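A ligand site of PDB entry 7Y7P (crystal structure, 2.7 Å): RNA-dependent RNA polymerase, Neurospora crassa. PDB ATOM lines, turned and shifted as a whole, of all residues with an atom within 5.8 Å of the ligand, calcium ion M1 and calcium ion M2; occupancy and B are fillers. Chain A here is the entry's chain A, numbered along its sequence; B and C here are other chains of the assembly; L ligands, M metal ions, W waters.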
ATOM      1  N   ARG A 295       6.563 -16.867 -17.767  1.00  0.00           N
ATOM      2  CA  ARG A 295       6.606 -18.334 -17.851  1.00  0.00           C
ATOM      3  C   ARG A 295       7.583 -18.817 -18.935  1.00  0.00           C
ATOM      4  O   ARG A 295       7.771 -20.039 -19.028  1.00  0.00           O
ATOM      5  CB  ARG A 295       5.192 -18.879 -18.022  1.00  0.00           C
ATOM      6  CG  ARG A 295       4.188 -18.346 -17.001  1.00  0.00           C
ATOM      7  CD  ARG A 295       4.670 -18.542 -15.592  1.00  0.00           C
ATOM      8  NE  ARG A 295       3.669 -18.117 -14.638  1.00  0.00           N
ATOM      9  CZ  ARG A 295       3.810 -18.194 -13.325  1.00  0.00           C
ATOM     10  NH1 ARG A 295       4.922 -18.681 -12.816  1.00  0.00           N
ATOM     11  NH2 ARG A 295       2.835 -17.784 -12.530  1.00  0.00           N
ATOM     12  N   ASP A 333       0.169 -26.110  -2.338  1.00  0.00           N
ATOM     13  CA  ASP A 333       0.632 -25.232  -3.410  1.00  0.00           C
ATOM     14  C   ASP A 333       1.942 -25.703  -4.031  1.00  0.00           C
ATOM     15  O   ASP A 333       3.006 -25.584  -3.424  1.00  0.00           O
ATOM     16  CB  ASP A 333       0.786 -23.797  -2.888  1.00  0.00           C
ATOM     17  CG  ASP A 333       0.853 -22.786  -4.002  1.00  0.00           C
ATOM     18  OD1 ASP A 333       0.851 -23.197  -5.180  1.00  0.00           O
ATOM     19  OD2 ASP A 333       0.900 -21.569  -3.709  1.00  0.00           O
ATOM     20  N   LYS A 367       4.944 -26.657 -12.527  1.00  0.00           N
ATOM     21  CA  LYS A 367       6.191 -26.311 -11.858  1.00  0.00           C
ATOM     22  C   LYS A 367       6.056 -26.595 -10.369  1.00  0.00           C
ATOM     23  O   LYS A 367       5.012 -26.292  -9.774  1.00  0.00           O
ATOM     24  CB  LYS A 367       6.564 -24.838 -12.090  1.00  0.00           C
ATOM     25  CG  LYS A 367       7.910 -24.427 -11.489  1.00  0.00           C
ATOM     26  CD  LYS A 367       8.023 -22.915 -11.325  1.00  0.00           C
ATOM     27  CE  LYS A 367       6.776 -22.332 -10.693  1.00  0.00           C
ATOM     28  NZ  LYS A 367       6.896 -22.234  -9.211  1.00  0.00           N
ATOM     29  N   SER A 388      -2.431 -25.498  -8.652  1.00  0.00           N
ATOM     30  CA  SER A 388      -1.359 -24.656  -8.126  1.00  0.00           C
ATOM     31  C   SER A 388      -0.039 -24.873  -8.856  1.00  0.00           C
ATOM     32  O   SER A 388       0.820 -23.977  -8.837  1.00  0.00           O
ATOM     33  CB  SER A 388      -1.172 -24.926  -6.629  1.00  0.00           C
ATOM     34  OG  SER A 388      -0.902 -26.293  -6.380  1.00  0.00           O
ATOM     35  N   LYS A 391       1.142 -23.629 -14.601  1.00  0.00           N
ATOM     36  CA  LYS A 391       1.249 -22.188 -14.777  1.00  0.00           C
ATOM     37  C   LYS A 391       0.541 -21.685 -16.034  1.00  0.00           C
ATOM     38  O   LYS A 391       0.327 -20.470 -16.156  1.00  0.00           O
ATOM     39  CB  LYS A 391       2.722 -21.766 -14.810  1.00  0.00           C
ATOM     40  CG  LYS A 391       3.448 -22.049 -13.504  1.00  0.00           C
ATOM     41  CD  LYS A 391       2.648 -21.561 -12.315  1.00  0.00           C
ATOM     42  CE  LYS A 391       3.183 -22.132 -11.015  1.00  0.00           C
ATOM     43  NZ  LYS A 391       2.358 -21.715  -9.849  1.00  0.00           N
ATOM     44  N   ARG A 586      11.910 -19.090   6.667  1.00  0.00           N
ATOM     45  CA  ARG A 586      12.348 -19.067   5.266  1.00  0.00           C
ATOM     46  C   ARG A 586      12.981 -17.702   5.000  1.00  0.00           C
ATOM     47  O   ARG A 586      12.676 -16.773   5.742  1.00  0.00           O
ATOM     48  CB  ARG A 586      11.136 -19.315   4.360  1.00  0.00           C
ATOM     49  CG  ARG A 586      11.453 -19.969   3.029  1.00  0.00           C
ATOM     50  CD  ARG A 586      10.179 -20.222   2.243  1.00  0.00           C
ATOM     51  NE  ARG A 586       9.589 -19.021   1.685  1.00  0.00           N
ATOM     52  CZ  ARG A 586       9.959 -18.447   0.549  1.00  0.00           C
ATOM     53  NH1 ARG A 586      10.931 -18.959  -0.182  1.00  0.00           N
ATOM     54  NH2 ARG A 586       9.344 -17.351   0.138  1.00  0.00           N
ATOM     55  N   SER A 587      13.858 -17.621   4.011  1.00  0.00           N
ATOM     56  CA  SER A 587      14.444 -16.315   3.613  1.00  0.00           C
ATOM     57  C   SER A 587      13.767 -15.900   2.311  1.00  0.00           C
ATOM     58  O   SER A 587      13.497 -16.792   1.496  1.00  0.00           O
ATOM     59  CB  SER A 587      15.926 -16.440   3.442  1.00  0.00           C
ATOM     60  OG  SER A 587      16.440 -15.300   2.770  1.00  0.00           O
ATOM     61  N   PRO A 588      13.450 -14.606   2.068  1.00  0.00           N
ATOM     62  CA  PRO A 588      13.735 -13.526   3.008  1.00  0.00           C
ATOM     63  C   PRO A 588      12.782 -13.506   4.207  1.00  0.00           C
ATOM     64  O   PRO A 588      11.613 -13.740   4.022  1.00  0.00           O
ATOM     65  CB  PRO A 588      13.528 -12.262   2.168  1.00  0.00           C
ATOM     66  CG  PRO A 588      13.474 -12.740   0.753  1.00  0.00           C
ATOM     67  CD  PRO A 588      12.832 -14.110   0.852  1.00  0.00           C
ATOM     68  N   SER A 628       6.884 -16.293   4.974  1.00  0.00           N
ATOM     69  CA  SER A 628       7.156 -15.352   3.856  1.00  0.00           C
ATOM     70  C   SER A 628       6.398 -15.692   2.578  1.00  0.00           C
ATOM     71  O   SER A 628       6.970 -15.511   1.501  1.00  0.00           O
ATOM     72  CB  SER A 628       8.626 -15.195   3.608  1.00  0.00           C
ATOM     73  OG  SER A 628       8.924 -13.908   3.092  1.00  0.00           O
ATOM     74  N   GLY A 629       5.123 -16.078   2.687  1.00  0.00           N
ATOM     75  CA  GLY A 629       4.328 -16.462   1.507  1.00  0.00           C
ATOM     76  C   GLY A 629       4.916 -17.641   0.775  1.00  0.00           C
ATOM     77  O   GLY A 629       4.932 -17.619  -0.469  1.00  0.00           O
ATOM     78  N   GLY A 630       5.377 -18.622   1.532  1.00  0.00           N
ATOM     79  CA  GLY A 630       6.049 -19.790   0.939  1.00  0.00           C
ATOM     80  C   GLY A 630       5.129 -20.825   0.366  1.00  0.00           C
ATOM     81  O   GLY A 630       3.932 -20.803   0.685  1.00  0.00           O
ATOM     82  N   ASP A 631       5.698 -21.743  -0.411  1.00  0.00           N
ATOM     83  CA  ASP A 631       4.900 -22.801  -1.062  1.00  0.00           C
ATOM     84  C   ASP A 631       5.673 -24.112  -1.001  1.00  0.00           C
ATOM     85  O   ASP A 631       6.682 -24.178  -0.311  1.00  0.00           O
ATOM     86  CB  ASP A 631       4.476 -22.443  -2.491  1.00  0.00           C
ATOM     87  CG  ASP A 631       5.494 -21.758  -3.366  1.00  0.00           C
ATOM     88  OD1 ASP A 631       6.670 -21.798  -3.027  1.00  0.00           O
ATOM     89  OD2 ASP A 631       5.082 -21.188  -4.392  1.00  0.00           O
ATOM     90  N   TYR A 632       5.149 -25.139  -1.658  1.00  0.00           N
ATOM     91  CA  TYR A 632       5.814 -26.461  -1.716  1.00  0.00           C
ATOM     92  C   TYR A 632       6.280 -26.686  -3.163  1.00  0.00           C
ATOM     93  O   TYR A 632       6.132 -27.791  -3.652  1.00  0.00           O
ATOM     94  CB  TYR A 632       4.871 -27.516  -1.150  1.00  0.00           C
ATOM     95  CG  TYR A 632       4.230 -27.135   0.160  1.00  0.00           C
ATOM     96  CD1 TYR A 632       4.901 -27.327   1.360  1.00  0.00           C
ATOM     97  CD2 TYR A 632       2.961 -26.598   0.212  1.00  0.00           C
ATOM     98  CE1 TYR A 632       4.330 -26.991   2.569  1.00  0.00           C
ATOM     99  CE2 TYR A 632       2.373 -26.242   1.407  1.00  0.00           C
ATOM    100  CZ  TYR A 632       3.051 -26.454   2.593  1.00  0.00           C
ATOM    101  OH  TYR A 632       2.486 -26.107   3.789  1.00  0.00           O
ATOM    102  N   ASP A 633       6.757 -25.638  -3.833  1.00  0.00           N
ATOM    103  CA  ASP A 633       7.165 -25.685  -5.266  1.00  0.00           C
ATOM    104  C   ASP A 633       8.685 -25.698  -5.461  1.00  0.00           C
ATOM    105  O   ASP A 633       9.128 -25.501  -6.596  1.00  0.00           O
ATOM    106  CB  ASP A 633       6.500 -24.542  -6.032  1.00  0.00           C
ATOM    107  CG  ASP A 633       7.135 -23.178  -5.893  1.00  0.00           C
ATOM    108  OD1 ASP A 633       8.027 -22.992  -5.050  1.00  0.00           O
ATOM    109  OD2 ASP A 633       6.697 -22.287  -6.629  1.00  0.00           O
ATOM    110  N   GLY A 634       9.461 -25.972  -4.419  1.00  0.00           N
ATOM    111  CA  GLY A 634      10.925 -25.889  -4.495  1.00  0.00           C
ATOM    112  C   GLY A 634      11.448 -25.106  -3.327  1.00  0.00           C
ATOM    113  O   GLY A 634      12.673 -24.968  -3.207  1.00  0.00           O
ATOM    114  N   ASP A 635      10.540 -24.603  -2.514  1.00  0.00           N
ATOM    115  CA  ASP A 635      10.913 -23.817  -1.321  1.00  0.00           C
ATOM    116  C   ASP A 635      11.660 -24.683  -0.296  1.00  0.00           C
ATOM    117  O   ASP A 635      11.328 -25.861  -0.172  1.00  0.00           O
ATOM    118  CB  ASP A 635       9.674 -23.245  -0.640  1.00  0.00           C
ATOM    119  CG  ASP A 635       9.136 -21.989  -1.281  1.00  0.00           C
ATOM    120  OD1 ASP A 635       9.306 -21.842  -2.496  1.00  0.00           O
ATOM    121  OD2 ASP A 635       8.545 -21.191  -0.551  1.00  0.00           O
ATOM    122  N   LEU A 706      14.101  -3.237  -5.036  1.00  0.00           N
ATOM    123  CA  LEU A 706      14.014  -4.249  -3.946  1.00  0.00           C
ATOM    124  C   LEU A 706      15.224  -4.092  -3.030  1.00  0.00           C
ATOM    125  O   LEU A 706      15.025  -4.081  -1.814  1.00  0.00           O
ATOM    126  CB  LEU A 706      13.998  -5.657  -4.552  1.00  0.00           C
ATOM    127  CG  LEU A 706      14.221  -6.803  -3.568  1.00  0.00           C
ATOM    128  CD1 LEU A 706      12.993  -7.016  -2.706  1.00  0.00           C
ATOM    129  CD2 LEU A 706      14.575  -8.082  -4.310  1.00  0.00           C
ATOM    130  N   GLY A 736       8.114  -7.431   0.170  1.00  0.00           N
ATOM    131  CA  GLY A 736       7.421  -8.671  -0.224  1.00  0.00           C
ATOM    132  C   GLY A 736       6.750  -8.535  -1.574  1.00  0.00           C
ATOM    133  O   GLY A 736       6.709  -9.510  -2.304  1.00  0.00           O
ATOM    134  N   VAL A 739       9.635  -8.167  -4.676  1.00  0.00           N
ATOM    135  CA  VAL A 739      10.341  -9.419  -5.101  1.00  0.00           C
ATOM    136  C   VAL A 739       9.486 -10.129  -6.144  1.00  0.00           C
ATOM    137  O   VAL A 739      10.061 -10.763  -7.038  1.00  0.00           O
ATOM    138  CB  VAL A 739      10.709 -10.305  -3.891  1.00  0.00           C
ATOM    139  CG1 VAL A 739       9.503 -10.805  -3.125  1.00  0.00           C
ATOM    140  CG2 VAL A 739      11.628 -11.448  -4.277  1.00  0.00           C
ATOM    141  N   ASP A 740       8.166  -9.996  -6.056  1.00  0.00           N
ATOM    142  CA  ASP A 740       7.234 -10.672  -6.984  1.00  0.00           C
ATOM    143  C   ASP A 740       6.841  -9.719  -8.109  1.00  0.00           C
ATOM    144  O   ASP A 740       5.816  -9.976  -8.743  1.00  0.00           O
ATOM    145  CB  ASP A 740       6.005 -11.143  -6.220  1.00  0.00           C
ATOM    146  CG  ASP A 740       6.321 -11.981  -5.001  1.00  0.00           C
ATOM    147  OD1 ASP A 740       7.337 -12.689  -5.035  1.00  0.00           O
ATOM    148  OD2 ASP A 740       5.544 -11.927  -4.038  1.00  0.00           O
ATOM    149  N   LYS A 743       6.355 -11.265 -11.946  1.00  0.00           N
ATOM    150  CA  LYS A 743       5.141 -12.103 -12.077  1.00  0.00           C
ATOM    151  C   LYS A 743       3.874 -11.291 -11.810  1.00  0.00           C
ATOM    152  O   LYS A 743       2.860 -11.567 -12.447  1.00  0.00           O
ATOM    153  CB  LYS A 743       5.250 -13.361 -11.212  1.00  0.00           C
ATOM    154  CG  LYS A 743       5.477 -14.654 -11.981  1.00  0.00           C
ATOM    155  CD  LYS A 743       6.150 -15.718 -11.154  1.00  0.00           C
ATOM    156  CE  LYS A 743       7.532 -16.079 -11.652  1.00  0.00           C
ATOM    157  NZ  LYS A 743       8.209 -17.025 -10.740  1.00  0.00           N
ATOM    158  P     C B   7      12.415 -21.645  -9.174  1.00  0.00           P
ATOM    159  OP1   C B   7      11.157 -22.413  -9.384  1.00  0.00           O
ATOM    160  OP2   C B   7      12.668 -20.413  -9.961  1.00  0.00           O
ATOM    161  O5'   C B   7      12.482 -21.281  -7.626  1.00  0.00           O
ATOM    162  C5'   C B   7      12.261 -22.266  -6.635  1.00  0.00           C
ATOM    163  C4'   C B   7      12.108 -21.646  -5.270  1.00  0.00           C
ATOM    164  O4'   C B   7      13.416 -21.284  -4.751  1.00  0.00           O
ATOM    165  C3'   C B   7      11.320 -20.348  -5.230  1.00  0.00           C
ATOM    166  O3'   C B   7       9.919 -20.546  -5.231  1.00  0.00           O
ATOM    167  C2'   C B   7      11.837 -19.688  -3.954  1.00  0.00           C
ATOM    168  O2'   C B   7      11.236 -20.272  -2.807  1.00  0.00           O
ATOM    169  C1'   C B   7      13.310 -20.106  -3.985  1.00  0.00           C
ATOM    170  N1    C B   7      14.179 -19.073  -4.609  1.00  0.00           N
ATOM    171  C2    C B   7      14.706 -18.061  -3.803  1.00  0.00           C
ATOM    172  O2    C B   7      14.440 -18.052  -2.594  1.00  0.00           O
ATOM    173  N3    C B   7      15.494 -17.113  -4.367  1.00  0.00           N
ATOM    174  C4    C B   7      15.764 -17.158  -5.685  1.00  0.00           C
ATOM    175  N4    C B   7      16.542 -16.202  -6.190  1.00  0.00           N
ATOM    176  C5    C B   7      15.227 -18.181  -6.519  1.00  0.00           C
ATOM    177  C6    C B   7      14.450 -19.109  -5.949  1.00  0.00           C
ATOM    178  P     U C   7      21.645  -4.982  -3.611  1.00  0.00           P
ATOM    179  OP1   U C   7      22.934  -4.583  -3.022  1.00  0.00           O
ATOM    180  OP2   U C   7      21.614  -5.692  -4.909  1.00  0.00           O
ATOM    181  O5'   U C   7      20.848  -5.843  -2.543  1.00  0.00           O
ATOM    182  C5'   U C   7      20.695  -5.393  -1.200  1.00  0.00           C
ATOM    183  C4'   U C   7      19.808  -6.339  -0.441  1.00  0.00           C
ATOM    184  O4'   U C   7      18.565  -6.523  -1.163  1.00  0.00           O
ATOM    185  C3'   U C   7      20.333  -7.763  -0.287  1.00  0.00           C
ATOM    186  O3'   U C   7      21.286  -7.930   0.754  1.00  0.00           O
ATOM    187  C2'   U C   7      19.048  -8.515   0.004  1.00  0.00           C
ATOM    188  O2'   U C   7      18.602  -8.326   1.325  1.00  0.00           O
ATOM    189  C1'   U C   7      18.077  -7.840  -0.961  1.00  0.00           C
ATOM    190  N1    U C   7      18.000  -8.511  -2.263  1.00  0.00           N
ATOM    191  C2    U C   7      17.301  -9.700  -2.323  1.00  0.00           C
ATOM    192  O2    U C   7      16.722 -10.189  -1.364  1.00  0.00           O
ATOM    193  N3    U C   7      17.276 -10.291  -3.557  1.00  0.00           N
ATOM    194  C4    U C   7      17.869  -9.837  -4.714  1.00  0.00           C
ATOM    195  O4    U C   7      17.749 -10.477  -5.753  1.00  0.00           O
ATOM    196  C5    U C   7      18.589  -8.609  -4.565  1.00  0.00           C
ATOM    197  C6    U C   7      18.626  -7.997  -3.378  1.00  0.00           C
ATOM    198  P     G C   8      22.384  -9.063   0.621  1.00  0.00           P
ATOM    199  OP1   G C   8      23.568  -8.715   1.495  1.00  0.00           O
ATOM    200  OP2   G C   8      22.706  -9.273  -0.836  1.00  0.00           O
ATOM    201  O5'   G C   8      21.668 -10.369   1.217  1.00  0.00           O
ATOM    202  C5'   G C   8      21.303 -10.379   2.613  1.00  0.00           C
ATOM    203  C4'   G C   8      20.224 -11.411   2.846  1.00  0.00           C
ATOM    204  O4'   G C   8      19.144 -11.221   1.896  1.00  0.00           O
ATOM    205  C3'   G C   8      20.629 -12.870   2.617  1.00  0.00           C
ATOM    206  O3'   G C   8      21.390 -13.406   3.694  1.00  0.00           O
ATOM    207  C2'   G C   8      19.244 -13.504   2.455  1.00  0.00           C
ATOM    208  O2'   G C   8      18.578 -13.653   3.685  1.00  0.00           O
ATOM    209  C1'   G C   8      18.564 -12.459   1.577  1.00  0.00           C
ATOM    210  N9    G C   8      18.728 -12.707   0.147  1.00  0.00           N
ATOM    211  C8    G C   8      19.576 -12.049  -0.697  1.00  0.00           C
ATOM    212  N7    G C   8      19.510 -12.492  -1.936  1.00  0.00           N
ATOM    213  C5    G C   8      18.563 -13.493  -1.891  1.00  0.00           C
ATOM    214  C6    G C   8      18.077 -14.328  -2.935  1.00  0.00           C
ATOM    215  O6    G C   8      18.403 -14.335  -4.124  1.00  0.00           O
ATOM    216  N1    G C   8      17.115 -15.221  -2.456  1.00  0.00           N
ATOM    217  C2    G C   8      16.683 -15.302  -1.163  1.00  0.00           C
ATOM    218  N2    G C   8      15.749 -16.218  -0.898  1.00  0.00           N
ATOM    219  N3    G C   8      17.127 -14.517  -0.180  1.00  0.00           N
ATOM    220  C4    G C   8      18.072 -13.646  -0.620  1.00  0.00           C
HETATM  221  P1  LIG L   1       7.925 -18.417  -6.420  1.00  0.00           P
HETATM  222  P2  LIG L   1       5.393 -17.345  -7.044  1.00  0.00           P
HETATM  223  P3  LIG L   1       4.540 -18.926  -9.260  1.00  0.00           P
HETATM  224  O1  LIG L   1       9.291 -18.444  -7.058  1.00  0.00           O
HETATM  225  O2  LIG L   1       5.269 -15.898  -6.664  1.00  0.00           O
HETATM  226  O3  LIG L   1       5.716 -18.884 -10.200  1.00  0.00           O
HETATM  227  O4  LIG L   1       7.262 -19.696  -5.993  1.00  0.00           O
HETATM  228  O5  LIG L   1       4.918 -18.410  -6.087  1.00  0.00           O
HETATM  229  O6  LIG L   1       3.187 -18.855  -9.928  1.00  0.00           O
HETATM  230  N1  LIG L   1       6.934 -17.612  -7.419  1.00  0.00           N
HETATM  231  O7  LIG L   1       4.654 -17.519  -8.478  1.00  0.00           O
HETATM  232  O8  LIG L   1       4.626 -19.990  -8.203  1.00  0.00           O
HETATM  233  O9  LIG L   1       7.980 -17.415  -5.161  1.00  0.00           O
HETATM  234  C1  LIG L   1       9.070 -16.501  -5.036  1.00  0.00           C
HETATM  235  C2  LIG L   1       9.350 -16.217  -3.558  1.00  0.00           C
HETATM  236  O10 LIG L   1      10.621 -16.763  -3.205  1.00  0.00           O
HETATM  237  C3  LIG L   1       9.420 -14.729  -3.281  1.00  0.00           C
HETATM  238  O11 LIG L   1       8.180 -14.243  -2.760  1.00  0.00           O
HETATM  239  C4  LIG L   1      10.525 -14.619  -2.252  1.00  0.00           C
HETATM  240  O12 LIG L   1      10.012 -14.803  -0.931  1.00  0.00           O
HETATM  241  C5  LIG L   1      11.449 -15.773  -2.597  1.00  0.00           C
HETATM  242  N2  LIG L   1      12.386 -15.258  -3.625  1.00  0.00           N
HETATM  243  C6  LIG L   1      12.382 -15.636  -4.919  1.00  0.00           C
HETATM  244  N3  LIG L   1      13.363 -14.997  -5.610  1.00  0.00           N
HETATM  245  C7  LIG L   1      13.995 -14.182  -4.750  1.00  0.00           C
HETATM  246  C8  LIG L   1      15.110 -13.222  -4.837  1.00  0.00           C
HETATM  247  N4  LIG L   1      15.763 -13.005  -6.007  1.00  0.00           N
HETATM  248  N5  LIG L   1      15.468 -12.575  -3.705  1.00  0.00           N
HETATM  249  C9  LIG L   1      14.834 -12.791  -2.541  1.00  0.00           C
HETATM  250  N6  LIG L   1      13.801 -13.638  -2.388  1.00  0.00           N
HETATM  251  C10 LIG L   1      13.348 -14.362  -3.443  1.00  0.00           C
HETATM  252 CA    CA M   1       7.983 -20.885  -4.106  1.00  0.00          CA
HETATM  253 CA    CA M   2       4.847 -20.604  -6.146  1.00  0.00          CA
HETATM  254 CA    CA M   3       4.601 -16.763  -2.814  1.00  0.00          CA
HETATM  255  O   HOH W   1       7.520 -19.541  -2.159  1.00  0.00           O
HETATM  256  O   HOH W   2       6.772 -15.646  -1.052  1.00  0.00           O
HETATM  257  O   HOH W   3       3.123 -22.568  -6.108  1.00  0.00           O
HETATM  258  O   HOH W   4       5.554 -14.619  -3.662  1.00  0.00           O
HETATM  259  O   HOH W   5      14.118 -14.576  -7.970  1.00  0.00           O
HETATM  260  O   HOH W   6       2.326 -20.190  -5.659  1.00  0.00           O
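Of the 24 residues printed, 4 come within 4 Å of calcium ion M1. The nearest printed residue that does not touch calcium ion M1 is Arg 586 (5.3 Å).
Calcium ion M2 is bound by the side-chain carboxylate (OD2) of Asp 631 (1.9 Å). An oxygen (O8) of the ligand binds calcium ion M2 (2.2 Å). Calcium ion M2 is bound by an oxygen (O5) of the ligand (2.2 Å). Calcium ion M2 is bound by OD2 of Asp 633 (2.5 Å). An oxygen (O4) of the ligand is bound to calcium ion M2, at 2.6 Å. Calcium ion M2 is bound by water W6. Water W3 is bound to calcium ion M2, at 2.6 Å. Calcium ion M2 has seven donor atoms within binding distance.
A nitrogen (N4) of the ligand sits at hydrogen-bond distance from N4 of C 7 of chain B, at 3.3 Å. An oxygen (O3) of the ligand lies within salt-bridge range of the guanidinium group (NH1) of Arg 295 (2.7 Å). The guanidinium group (NH2) of Arg 586 is in hydrogen-bond range of an oxygen (O12) of the ligand (2.8 Å). OD1 of Asp 740 is in hydrogen-bond range of O11 of the ligand, 2.9 Å away. O4 of U 7 of chain C sits at hydrogen-bond distance from N4 of the ligand, at 3.2 Å. NZ of Lys 391 is in salt-bridge range of O6 of the ligand. NZ of Lys 743 is in salt-bridge range of O3 of the ligand (3.2 Å). The side-chain amino group (NZ) of Lys 367 lies within salt-bridge range of an oxygen (O3) of the ligand.
O2' of C 7 of chain B lies within hydrogen-bond range of the guanidinium group (NH1) of Arg 586, at 3.0 Å. The side-chain carboxylate of Asp 635 is in salt-bridge range of the guanidinium group of Arg 586, at 3.3 Å. The side-chain carboxylate of Asp 633 lies close to the side-chain amino group of Lys 367 (2.6 Å). NH2 of Arg 586 is in hydrogen-bond range of O of Ser 628 (3.3 Å). The backbone carbonyl oxygen (O) of Ser 388 lies within hydrogen-bond range of the side-chain amino group (NZ) of Lys 391, at 2.9 Å. O2' of G 8 of chain C lies within hydrogen-bond range of the side-chain hydroxyl (OG) of Ser 587 (2.8 Å). The backbone carbonyl oxygen (O) of Pro 588 sits at hydrogen-bond distance from the side-chain hydroxyl (OG) of Ser 628 (2.9 Å).
Calcium ion M1 is bound by the side-chain carboxylate (OD1) of Asp 631 (1.9 Å), O3' of C 7 of chain B (2.3 Å), the side-chain carboxylate (OD1) of Asp 635 (2.3 Å), the side-chain carboxylate (OD1) of Asp 633 (2.3 Å), an oxygen (O4) of the ligand (2.3 Å) and water W1 (2.4 Å). Slightly farther from calcium ion M1 lies the side-chain carboxylate (OD2) of Asp 631 (2.9 Å).
Water W1 bridges the side-chain carboxylate of Asp 635 (2.5 Å) and the backbone NH of Asp 631 (3.4 Å). Water W5 lies within hydrogen-bond range of a nitrogen (N3) of the ligand and N4 of C 7 of chain B. Water W2 lies within hydrogen-bond range of O of Ser 628 (2.6 Å), O11 of the ligand (2.6 Å) and NH2 of Arg 586 (3.3 Å). Water W4 lies within hydrogen-bond range of the side-chain carboxylate of Asp 740 and an oxygen (O11) of the ligand.
N1 of G 8 of chain C sits close to N5 of the ligand (3.4 Å). Pro 588 touches the ligand. Ser 628 touches the ligand. CG2 of Val 739 touches C10 of the ligand, at 3.5 Å. Hydrophobic or aromatic side chains within 4 Å of the ligand: Pro 588 and Val 739. Within 4 Å of the ligand: Arg 295, Lys 367, Lys 391, Arg 586, Pro 588, Ser 628, Asp 631, Asp 633, Val 739, Asp 740, Lys 743, C 7 of chain B, U 7 of chain C and G 8 of chain C. The nearest printed residue that does not touch the ligand is Asp 635 (4.6 Å).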
